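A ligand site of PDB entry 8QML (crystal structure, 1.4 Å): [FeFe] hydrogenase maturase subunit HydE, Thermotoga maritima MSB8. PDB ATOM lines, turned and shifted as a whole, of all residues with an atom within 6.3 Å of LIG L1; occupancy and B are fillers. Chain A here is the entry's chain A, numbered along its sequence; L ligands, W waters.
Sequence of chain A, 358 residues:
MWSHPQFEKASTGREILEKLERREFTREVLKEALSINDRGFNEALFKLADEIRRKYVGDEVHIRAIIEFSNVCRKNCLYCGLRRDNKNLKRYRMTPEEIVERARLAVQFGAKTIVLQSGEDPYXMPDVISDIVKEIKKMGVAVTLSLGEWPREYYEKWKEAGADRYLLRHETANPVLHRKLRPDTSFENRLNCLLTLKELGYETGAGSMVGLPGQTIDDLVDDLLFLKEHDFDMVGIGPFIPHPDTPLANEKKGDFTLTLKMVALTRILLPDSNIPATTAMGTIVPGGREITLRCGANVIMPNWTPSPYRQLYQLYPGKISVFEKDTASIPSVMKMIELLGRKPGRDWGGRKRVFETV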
ATOM      1  N   VAL A  72     -21.123 -19.756  11.456  1.00  0.00           N
ATOM      2  CA  VAL A  72     -20.582 -19.666  10.097  1.00  0.00           C
ATOM      3  C   VAL A  72     -20.068 -21.049   9.728  1.00  0.00           C
ATOM      4  O   VAL A  72     -19.377 -21.695  10.523  1.00  0.00           O
ATOM      5  CB  VAL A  72     -19.449 -18.652  10.091  1.00  0.00           C
ATOM      6  CG1 VAL A  72     -18.734 -18.731   8.750  1.00  0.00           C
ATOM      7  CG2 VAL A  72     -20.000 -17.306  10.396  1.00  0.00           C
ATOM      8  N   CYS A  73     -20.348 -21.523   8.528  1.00  0.00           N
ATOM      9  CA  CYS A  73     -19.775 -22.783   8.113  1.00  0.00           C
ATOM     10  C   CYS A  73     -19.429 -22.753   6.658  1.00  0.00           C
ATOM     11  O   CYS A  73     -20.220 -22.294   5.840  1.00  0.00           O
ATOM     12  CB  CYS A  73     -20.766 -23.936   8.281  1.00  0.00           C
ATOM     13  SG  CYS A  73     -19.916 -25.503   8.169  1.00  0.00           S
ATOM     14  N   ARG A  74     -18.278 -23.343   6.350  1.00  0.00           N
ATOM     15  CA  ARG A  74     -17.831 -23.434   4.983  1.00  0.00           C
ATOM     16  C   ARG A  74     -18.328 -24.688   4.293  1.00  0.00           C
ATOM     17  O   ARG A  74     -18.165 -24.803   3.074  1.00  0.00           O
ATOM     18  CB  ARG A  74     -16.321 -23.442   4.971  1.00  0.00           C
ATOM     19  CG  ARG A  74     -15.797 -24.731   5.552  1.00  0.00           C
ATOM     20  CD  ARG A  74     -14.267 -24.692   5.673  1.00  0.00           C
ATOM     21  NE  ARG A  74     -13.769 -25.874   6.365  1.00  0.00           N
ATOM     22  CZ  ARG A  74     -12.515 -26.287   6.319  1.00  0.00           C
ATOM     23  NH1 ARG A  74     -11.599 -25.639   5.633  1.00  0.00           N
ATOM     24  NH2 ARG A  74     -12.162 -27.353   7.030  1.00  0.00           N
ATOM     25  N   LYS A  75     -18.905 -25.659   5.027  1.00  0.00           N
ATOM     26  CA  LYS A  75     -19.424 -26.858   4.412  1.00  0.00           C
ATOM     27  C   LYS A  75     -20.909 -26.728   4.155  1.00  0.00           C
ATOM     28  O   LYS A  75     -21.583 -25.758   4.546  1.00  0.00           O
ATOM     29  CB  LYS A  75     -19.133 -28.085   5.276  1.00  0.00           C
ATOM     30  CG  LYS A  75     -17.672 -28.507   5.265  1.00  0.00           C
ATOM     31  CD  LYS A  75     -17.439 -29.816   6.022  1.00  0.00           C
ATOM     32  CE  LYS A  75     -16.145 -30.428   5.541  1.00  0.00           C
ATOM     33  NZ  LYS A  75     -14.930 -29.594   5.642  1.00  0.00           N
ATOM     34  N   ASN A  76     -21.427 -27.734   3.468  1.00  0.00           N
ATOM     35  CA  ASN A  76     -22.764 -27.652   2.910  1.00  0.00           C
ATOM     36  C   ASN A  76     -23.511 -28.941   3.170  1.00  0.00           C
ATOM     37  O   ASN A  76     -24.290 -29.412   2.331  1.00  0.00           O
ATOM     38  CB  ASN A  76     -22.694 -27.348   1.423  1.00  0.00           C
ATOM     39  CG  ASN A  76     -23.890 -26.578   0.903  1.00  0.00           C
ATOM     40  OD1 ASN A  76     -24.559 -25.824   1.643  1.00  0.00           O
ATOM     41  ND2 ASN A  76     -24.106 -26.709  -0.409  1.00  0.00           N
ATOM     42  N   CYS A  77     -23.247 -29.562   4.305  1.00  0.00           N
ATOM     43  CA  CYS A  77     -23.926 -30.826   4.609  1.00  0.00           C
ATOM     44  C   CYS A  77     -25.437 -30.709   4.391  1.00  0.00           C
ATOM     45  O   CYS A  77     -26.055 -29.729   4.803  1.00  0.00           O
ATOM     46  CB  CYS A  77     -23.657 -31.233   6.054  1.00  0.00           C
ATOM     47  SG  CYS A  77     -21.931 -31.262   6.474  1.00  0.00           S
ATOM     48  N   LEU A  78     -26.023 -31.749   3.765  1.00  0.00           N
ATOM     49  CA  LEU A  78     -27.382 -31.650   3.280  1.00  0.00           C
ATOM     50  C   LEU A  78     -28.389 -31.551   4.383  1.00  0.00           C
ATOM     51  O   LEU A  78     -29.505 -31.076   4.170  1.00  0.00           O
ATOM     52  CB  LEU A  78     -27.743 -32.845   2.389  1.00  0.00           C
ATOM     53  CG  LEU A  78     -27.579 -32.540   0.905  1.00  0.00           C
ATOM     54  CD1 LEU A  78     -26.135 -32.197   0.589  1.00  0.00           C
ATOM     55  CD2 LEU A  78     -28.057 -33.769   0.098  1.00  0.00           C
ATOM     56  N   TYR A  79     -28.069 -32.118   5.532  1.00  0.00           N
ATOM     57  CA  TYR A  79     -29.003 -32.151   6.667  1.00  0.00           C
ATOM     58  C   TYR A  79     -28.939 -30.913   7.545  1.00  0.00           C
ATOM     59  O   TYR A  79     -29.878 -30.686   8.324  1.00  0.00           O
ATOM     60  CB  TYR A  79     -28.695 -33.391   7.523  1.00  0.00           C
ATOM     61  CG  TYR A  79     -27.236 -33.626   7.840  1.00  0.00           C
ATOM     62  CD1 TYR A  79     -26.596 -32.884   8.796  1.00  0.00           C
ATOM     63  CD2 TYR A  79     -26.497 -34.507   7.047  1.00  0.00           C
ATOM     64  CE1 TYR A  79     -25.195 -33.055   9.095  1.00  0.00           C
ATOM     65  CE2 TYR A  79     -25.154 -34.701   7.305  1.00  0.00           C
ATOM     66  CZ  TYR A  79     -24.514 -33.970   8.277  1.00  0.00           C
ATOM     67  OH  TYR A  79     -23.186 -34.141   8.527  1.00  0.00           O
ATOM     68  N   CYS A  80     -27.888 -30.106   7.465  1.00  0.00           N
ATOM     69  CA  CYS A  80     -27.552 -29.171   8.526  1.00  0.00           C
ATOM     70  C   CYS A  80     -28.082 -27.776   8.253  1.00  0.00           C
ATOM     71  O   CYS A  80     -27.819 -27.220   7.182  1.00  0.00           O
ATOM     72  CB  CYS A  80     -26.042 -29.115   8.756  1.00  0.00           C
ATOM     73  SG  CYS A  80     -25.633 -28.025  10.089  1.00  0.00           S
ATOM     74  N   GLY A  81     -28.781 -27.175   9.229  1.00  0.00           N
ATOM     75  CA  GLY A  81     -29.288 -25.810   9.033  1.00  0.00           C
ATOM     76  C   GLY A  81     -28.189 -24.752   8.886  1.00  0.00           C
ATOM     77  O   GLY A  81     -28.480 -23.658   8.381  1.00  0.00           O
ATOM     78  N   LEU A  82     -26.962 -25.052   9.275  1.00  0.00           N
ATOM     79  CA  LEU A  82     -25.853 -24.089   9.159  1.00  0.00           C
ATOM     80  C   LEU A  82     -25.138 -24.217   7.833  1.00  0.00           C
ATOM     81  O   LEU A  82     -24.162 -23.493   7.581  1.00  0.00           O
ATOM     82  CB  LEU A  82     -24.832 -24.245  10.307  1.00  0.00           C
ATOM     83  CG  LEU A  82     -25.455 -24.229  11.703  1.00  0.00           C
ATOM     84  CD1 LEU A  82     -24.306 -24.117  12.738  1.00  0.00           C
ATOM     85  CD2 LEU A  82     -26.477 -23.131  11.909  1.00  0.00           C
ATOM     86  N   ARG A  83     -25.608 -25.105   6.973  1.00  0.00           N
ATOM     87  CA  ARG A  83     -24.909 -25.336   5.709  1.00  0.00           C
ATOM     88  C   ARG A  83     -24.731 -24.019   4.966  1.00  0.00           C
ATOM     89  O   ARG A  83     -25.530 -23.077   5.053  1.00  0.00           O
ATOM     90  CB  ARG A  83     -25.655 -26.331   4.841  1.00  0.00           C
ATOM     91  CG  ARG A  83     -27.007 -25.816   4.491  1.00  0.00           C
ATOM     92  CD  ARG A  83     -27.919 -26.939   3.996  1.00  0.00           C
ATOM     93  NE  ARG A  83     -27.231 -27.812   3.048  1.00  0.00           N
ATOM     94  CZ  ARG A  83     -27.269 -27.603   1.737  1.00  0.00           C
ATOM     95  NH1 ARG A  83     -28.024 -26.645   1.236  1.00  0.00           N
ATOM     96  NH2 ARG A  83     -26.615 -28.422   0.912  1.00  0.00           N
ATOM     97  N   ARG A  84     -23.637 -23.969   4.227  1.00  0.00           N
ATOM     98  CA  ARG A  84     -23.275 -22.679   3.641  1.00  0.00           C
ATOM     99  C   ARG A  84     -24.339 -22.109   2.711  1.00  0.00           C
ATOM    100  O   ARG A  84     -24.486 -20.898   2.635  1.00  0.00           O
ATOM    101  CB  ARG A  84     -21.945 -22.704   2.903  1.00  0.00           C
ATOM    102  CG  ARG A  84     -21.906 -23.506   1.710  1.00  0.00           C
ATOM    103  CD  ARG A  84     -20.568 -23.248   1.038  1.00  0.00           C
ATOM    104  NE  ARG A  84     -20.563 -24.020  -0.183  1.00  0.00           N
ATOM    105  CZ  ARG A  84     -20.188 -25.298  -0.272  1.00  0.00           C
ATOM    106  NH1 ARG A  84     -19.574 -25.912   0.727  1.00  0.00           N
ATOM    107  NH2 ARG A  84     -20.505 -25.981  -1.363  1.00  0.00           N
ATOM    108  N   SER A 118     -18.862 -25.139  16.845  1.00  0.00           N
ATOM    109  CA  SER A 118     -19.229 -24.122  15.878  1.00  0.00           C
ATOM    110  C   SER A 118     -19.407 -24.824  14.532  1.00  0.00           C
ATOM    111  O   SER A 118     -19.047 -25.988  14.364  1.00  0.00           O
ATOM    112  CB  SER A 118     -18.077 -23.106  15.789  1.00  0.00           C
ATOM    113  OG  SER A 118     -16.884 -23.730  15.297  1.00  0.00           O
ATOM    114  N   GLY A 119     -19.942 -24.065  13.563  1.00  0.00           N
ATOM    115  CA  GLY A 119     -19.745 -24.440  12.161  1.00  0.00           C
ATOM    116  C   GLY A 119     -18.265 -24.456  11.825  1.00  0.00           C
ATOM    117  O   GLY A 119     -17.423 -24.000  12.594  1.00  0.00           O
ATOM    118  N   GLU A 120     -17.969 -24.984  10.648  1.00  0.00           N
ATOM    119  CA  GLU A 120     -16.559 -24.940  10.218  1.00  0.00           C
ATOM    120  C   GLU A 120     -16.289 -23.517   9.773  1.00  0.00           C
ATOM    121  O   GLU A 120     -16.340 -23.212   8.578  1.00  0.00           O
ATOM    122  CB  GLU A 120     -16.272 -25.929   9.118  1.00  0.00           C
ATOM    123  CG  GLU A 120     -16.221 -27.367   9.718  1.00  0.00           C
ATOM    124  CD  GLU A 120     -15.635 -28.340   8.735  1.00  0.00           C
ATOM    125  OE1 GLU A 120     -15.117 -27.908   7.691  1.00  0.00           O
ATOM    126  OE2 GLU A 120     -15.681 -29.557   9.011  1.00  0.00           O
ATOM    127  N   GLY A 148     -15.394 -29.471  13.749  1.00  0.00           N
ATOM    128  CA  GLY A 148     -15.401 -30.088  12.429  1.00  0.00           C
ATOM    129  C   GLY A 148     -14.036 -30.595  12.012  1.00  0.00           C
ATOM    130  O   GLY A 148     -13.159 -30.914  12.834  1.00  0.00           O
ATOM    131  N   GLU A 171     -21.192 -39.409  11.809  1.00  0.00           N
ATOM    132  CA  GLU A 171     -22.445 -39.125  11.090  1.00  0.00           C
ATOM    133  C   GLU A 171     -23.144 -40.353  10.549  1.00  0.00           C
ATOM    134  O   GLU A 171     -24.329 -40.586  10.801  1.00  0.00           O
ATOM    135  CB  GLU A 171     -22.295 -38.047   9.982  1.00  0.00           C
ATOM    136  CG  GLU A 171     -21.468 -36.880  10.507  1.00  0.00           C
ATOM    137  CD  GLU A 171     -22.130 -36.030  11.561  1.00  0.00           C
ATOM    138  OE1 GLU A 171     -23.214 -36.382  12.086  1.00  0.00           O
ATOM    139  OE2 GLU A 171     -21.520 -34.988  11.846  1.00  0.00           O
ATOM    140  N   ARG A 182     -22.705 -35.185   2.735  1.00  0.00           N
ATOM    141  CA  ARG A 182     -21.654 -34.253   3.147  1.00  0.00           C
ATOM    142  C   ARG A 182     -20.769 -34.033   1.936  1.00  0.00           C
ATOM    143  O   ARG A 182     -19.674 -34.568   1.849  1.00  0.00           O
ATOM    144  CB  ARG A 182     -20.877 -34.804   4.329  1.00  0.00           C
ATOM    145  CG  ARG A 182     -21.868 -35.224   5.421  1.00  0.00           C
ATOM    146  CD  ARG A 182     -21.118 -35.627   6.671  1.00  0.00           C
ATOM    147  NE  ARG A 182     -20.521 -34.463   7.275  1.00  0.00           N
ATOM    148  CZ  ARG A 182     -19.232 -34.234   7.414  1.00  0.00           C
ATOM    149  NH1 ARG A 182     -18.323 -35.175   7.171  1.00  0.00           N
ATOM    150  NH2 ARG A 182     -18.822 -33.016   7.783  1.00  0.00           N
ATOM    151  N   ARG A 190     -13.450 -38.092   7.398  1.00  0.00           N
ATOM    152  CA  ARG A 190     -13.994 -38.015   8.741  1.00  0.00           C
ATOM    153  C   ARG A 190     -13.272 -38.989   9.635  1.00  0.00           C
ATOM    154  O   ARG A 190     -12.860 -38.631  10.730  1.00  0.00           O
ATOM    155  CB  ARG A 190     -15.476 -38.432   8.709  1.00  0.00           C
ATOM    156  CG  ARG A 190     -16.316 -37.949   9.892  1.00  0.00           C
ATOM    157  CD  ARG A 190     -16.380 -36.444   9.915  1.00  0.00           C
ATOM    158  NE  ARG A 190     -17.437 -36.015  10.811  1.00  0.00           N
ATOM    159  CZ  ARG A 190     -17.697 -34.737  11.049  1.00  0.00           C
ATOM    160  NH1 ARG A 190     -17.121 -33.772  10.322  1.00  0.00           N
ATOM    161  NH2 ARG A 190     -18.537 -34.428  12.035  1.00  0.00           N
ATOM    162  N   TYR A 313     -28.298 -20.621  16.260  1.00  0.00           N
ATOM    163  CA  TYR A 313     -27.508 -21.819  16.029  1.00  0.00           C
ATOM    164  C   TYR A 313     -28.478 -22.968  15.869  1.00  0.00           C
ATOM    165  O   TYR A 313     -28.768 -23.692  16.808  1.00  0.00           O
ATOM    166  CB  TYR A 313     -26.498 -22.028  17.152  1.00  0.00           C
ATOM    167  CG  TYR A 313     -25.485 -23.076  16.871  1.00  0.00           C
ATOM    168  CD1 TYR A 313     -24.271 -22.739  16.265  1.00  0.00           C
ATOM    169  CD2 TYR A 313     -25.716 -24.376  17.220  1.00  0.00           C
ATOM    170  CE1 TYR A 313     -23.310 -23.693  16.000  1.00  0.00           C
ATOM    171  CE2 TYR A 313     -24.769 -25.354  17.000  1.00  0.00           C
ATOM    172  CZ  TYR A 313     -23.566 -24.988  16.402  1.00  0.00           C
ATOM    173  OH  TYR A 313     -22.590 -25.952  16.180  1.00  0.00           O
ATOM    174  N   LEU A 315     -28.972 -26.074  14.050  1.00  0.00           N
ATOM    175  CA  LEU A 315     -28.634 -27.226  13.216  1.00  0.00           C
ATOM    176  C   LEU A 315     -29.889 -27.900  12.712  1.00  0.00           C
ATOM    177  O   LEU A 315     -29.971 -28.359  11.565  1.00  0.00           O
ATOM    178  CB  LEU A 315     -27.891 -28.252  14.086  1.00  0.00           C
ATOM    179  CG  LEU A 315     -26.685 -27.723  14.804  1.00  0.00           C
ATOM    180  CD1 LEU A 315     -26.228 -28.812  15.745  1.00  0.00           C
ATOM    181  CD2 LEU A 315     -25.629 -27.507  13.691  1.00  0.00           C
HETATM  182 FE1  LIG L   1     -23.467 -28.264   9.792  1.00  0.00          FE
HETATM  183 FE2  LIG L   1     -21.191 -27.175   8.894  1.00  0.00          FE
HETATM  184 FE3  LIG L   1     -21.829 -29.756   8.241  1.00  0.00          FE
HETATM  185 FE4  LIG L   1     -21.045 -29.135  10.916  1.00  0.00          FE
HETATM  186  S1  LIG L   1     -19.806 -29.015   8.943  1.00  0.00           S
HETATM  187  S2  LIG L   1     -22.838 -30.419  10.190  1.00  0.00           S
HETATM  188  S3  LIG L   1     -22.009 -27.009  10.993  1.00  0.00           S
HETATM  189  S4  LIG L   1     -22.935 -27.859   7.602  1.00  0.00           S
HETATM  190  N1  LG2 L   2     -19.448 -28.340  12.383  1.00  0.00           N
HETATM  191  C1  LG2 L   2     -19.178 -29.388  13.386  1.00  0.00           C
HETATM  192  C2  LG2 L   2     -19.916 -29.172  14.701  1.00  0.00           C
HETATM  193  C3  LG2 L   2     -21.394 -28.741  14.633  1.00  0.00           C
HETATM  194  S1  LG2 L   2     -22.549 -29.925  13.881  1.00  0.00           S
HETATM  195  C4  LG2 L   2     -19.366 -30.753  12.795  1.00  0.00           C
HETATM  196  O1  LG2 L   2     -19.985 -30.935  11.722  1.00  0.00           O
HETATM  197  O2  LG2 L   2     -18.837 -31.710  13.391  1.00  0.00           O
HETATM  198  C5  LG2 L   2     -22.788 -31.018  15.307  1.00  0.00           C
HETATM  199  C6  LG2 L   2     -23.657 -32.254  15.002  1.00  0.00           C
HETATM  200  O3  LG2 L   2     -24.989 -31.834  14.782  1.00  0.00           O
HETATM  201  C7  LG2 L   2     -23.302 -32.950  13.695  1.00  0.00           C
HETATM  202  O4  LG2 L   2     -22.222 -33.828  13.977  1.00  0.00           O
HETATM  203  C8  LG2 L   2     -24.602 -33.651  13.331  1.00  0.00           C
HETATM  204  O5  LG2 L   2     -24.629 -35.033  13.688  1.00  0.00           O
HETATM  205  C9  LG2 L   2     -25.666 -32.877  14.139  1.00  0.00           C
HETATM  206  N2  LG2 L   2     -26.697 -32.349  13.254  1.00  0.00           N
HETATM  207  C10 LG2 L   2     -26.506 -31.464  12.169  1.00  0.00           C
HETATM  208  N3  LG2 L   2     -27.656 -31.282  11.551  1.00  0.00           N
HETATM  209  C11 LG2 L   2     -28.608 -32.080  12.167  1.00  0.00           C
HETATM  210  C12 LG2 L   2     -29.974 -32.271  11.943  1.00  0.00           C
HETATM  211  N4  LG2 L   2     -30.653 -31.681  10.937  1.00  0.00           N
HETATM  212  N5  LG2 L   2     -30.668 -33.146  12.743  1.00  0.00           N
HETATM  213  C13 LG2 L   2     -30.029 -33.799  13.776  1.00  0.00           C
HETATM  214  N6  LG2 L   2     -28.688 -33.598  14.044  1.00  0.00           N
HETATM  215  C14 LG2 L   2     -27.983 -32.746  13.228  1.00  0.00           C
HETATM  216  O   HOH W   1     -21.135 -33.033  10.028  1.00  0.00           O
HETATM  217  O   HOH W   2     -17.571 -31.087  10.046  1.00  0.00           O
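FE1 of LIG L1 is bound by SG of Cys 80 (2.2 Å). SG of Cys 73 is bound to FE2 of LIG L1. A sulfur (S4) of LIG L1 lies close to the backbone NH of Cys 77, 3.7 Å away. FE3 of LIG L1 is bound by SG of Cys 77 (2.3 Å). O of Tyr 79 sits at hydrogen-bond distance from N4 of LG2 L2 (2.9 Å). O of Leu 315 lies within hydrogen-bond range of N4 of LG2 L2 (3.4 Å). O of Ser 118 sits close to N1 of LG2 L2 (3.1 Å). The side-chain carboxylate of Glu 171 lies within hydrogen-bond range of an oxygen (O4) of LG2 L2, at 2.5 Å. The guanidinium group (NH2) of Arg 190 is in salt-bridge range of an oxygen (O2) of LG2 L2 (3.1 Å).
O1 of LG2 L2 is bound to FE4 of LIG L1 (2.2 Å).
SG of Cys 73 lies close to N of Lys 75, at 3.3 Å. N of Glu 120 lies close to SG of Cys 73 (3.2 Å). The side-chain sulfur (SG) of Cys 77 sits close to the side-chain hydroxyl (OH) of Tyr 79, at 3.8 Å. The side-chain sulfur of Cys 77 sits close to the guanidinium group of Arg 182 (3.6 Å). The side-chain hydroxyl of Tyr 79 sits at hydrogen-bond distance from the guanidinium group of Arg 182, at 3.0 Å. O of Asn 76 sits at hydrogen-bond distance from NH2 of Arg 83 (2.9 Å). NZ of Lys 75 is in salt-bridge range of OE1 of Glu 120, 2.7 Å away. The backbone carbonyl oxygen of Lys 75 lies within hydrogen-bond range of the backbone NH of Arg 84, at 2.7 Å.
Merely in contact with LIG L1: Gly 119 (3.6 Å), Tyr 79 (3.7 Å), Arg 83 (3.7 Å) and Lys 75 (3.8 Å). Hydrophobic or aromatic side chains that line LIG L1: Tyr 79. Seven residues have an atom within 4 Å of LIG L1: Cys 73, Lys 75, Cys 77, Tyr 79, Cys 80, Arg 83 and Gly 119. The nearest printed residue that does not touch LIG L1 is Leu 82 (4.01 Å).
Water W1 lies within hydrogen-bond range of the side-chain carboxylate of Glu 171, the side-chain hydroxyl of Tyr 79, a sulfur (S2) of LIG L1 and the guanidinium group of Arg 182. Water W2 lies within hydrogen-bond range of OE2 of Glu 120 (2.6 Å), NH1 of Arg 190 (2.7 Å), NH2 of Arg 182 (3.2 Å) and S1 of LIG L1 (3.2 Å).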
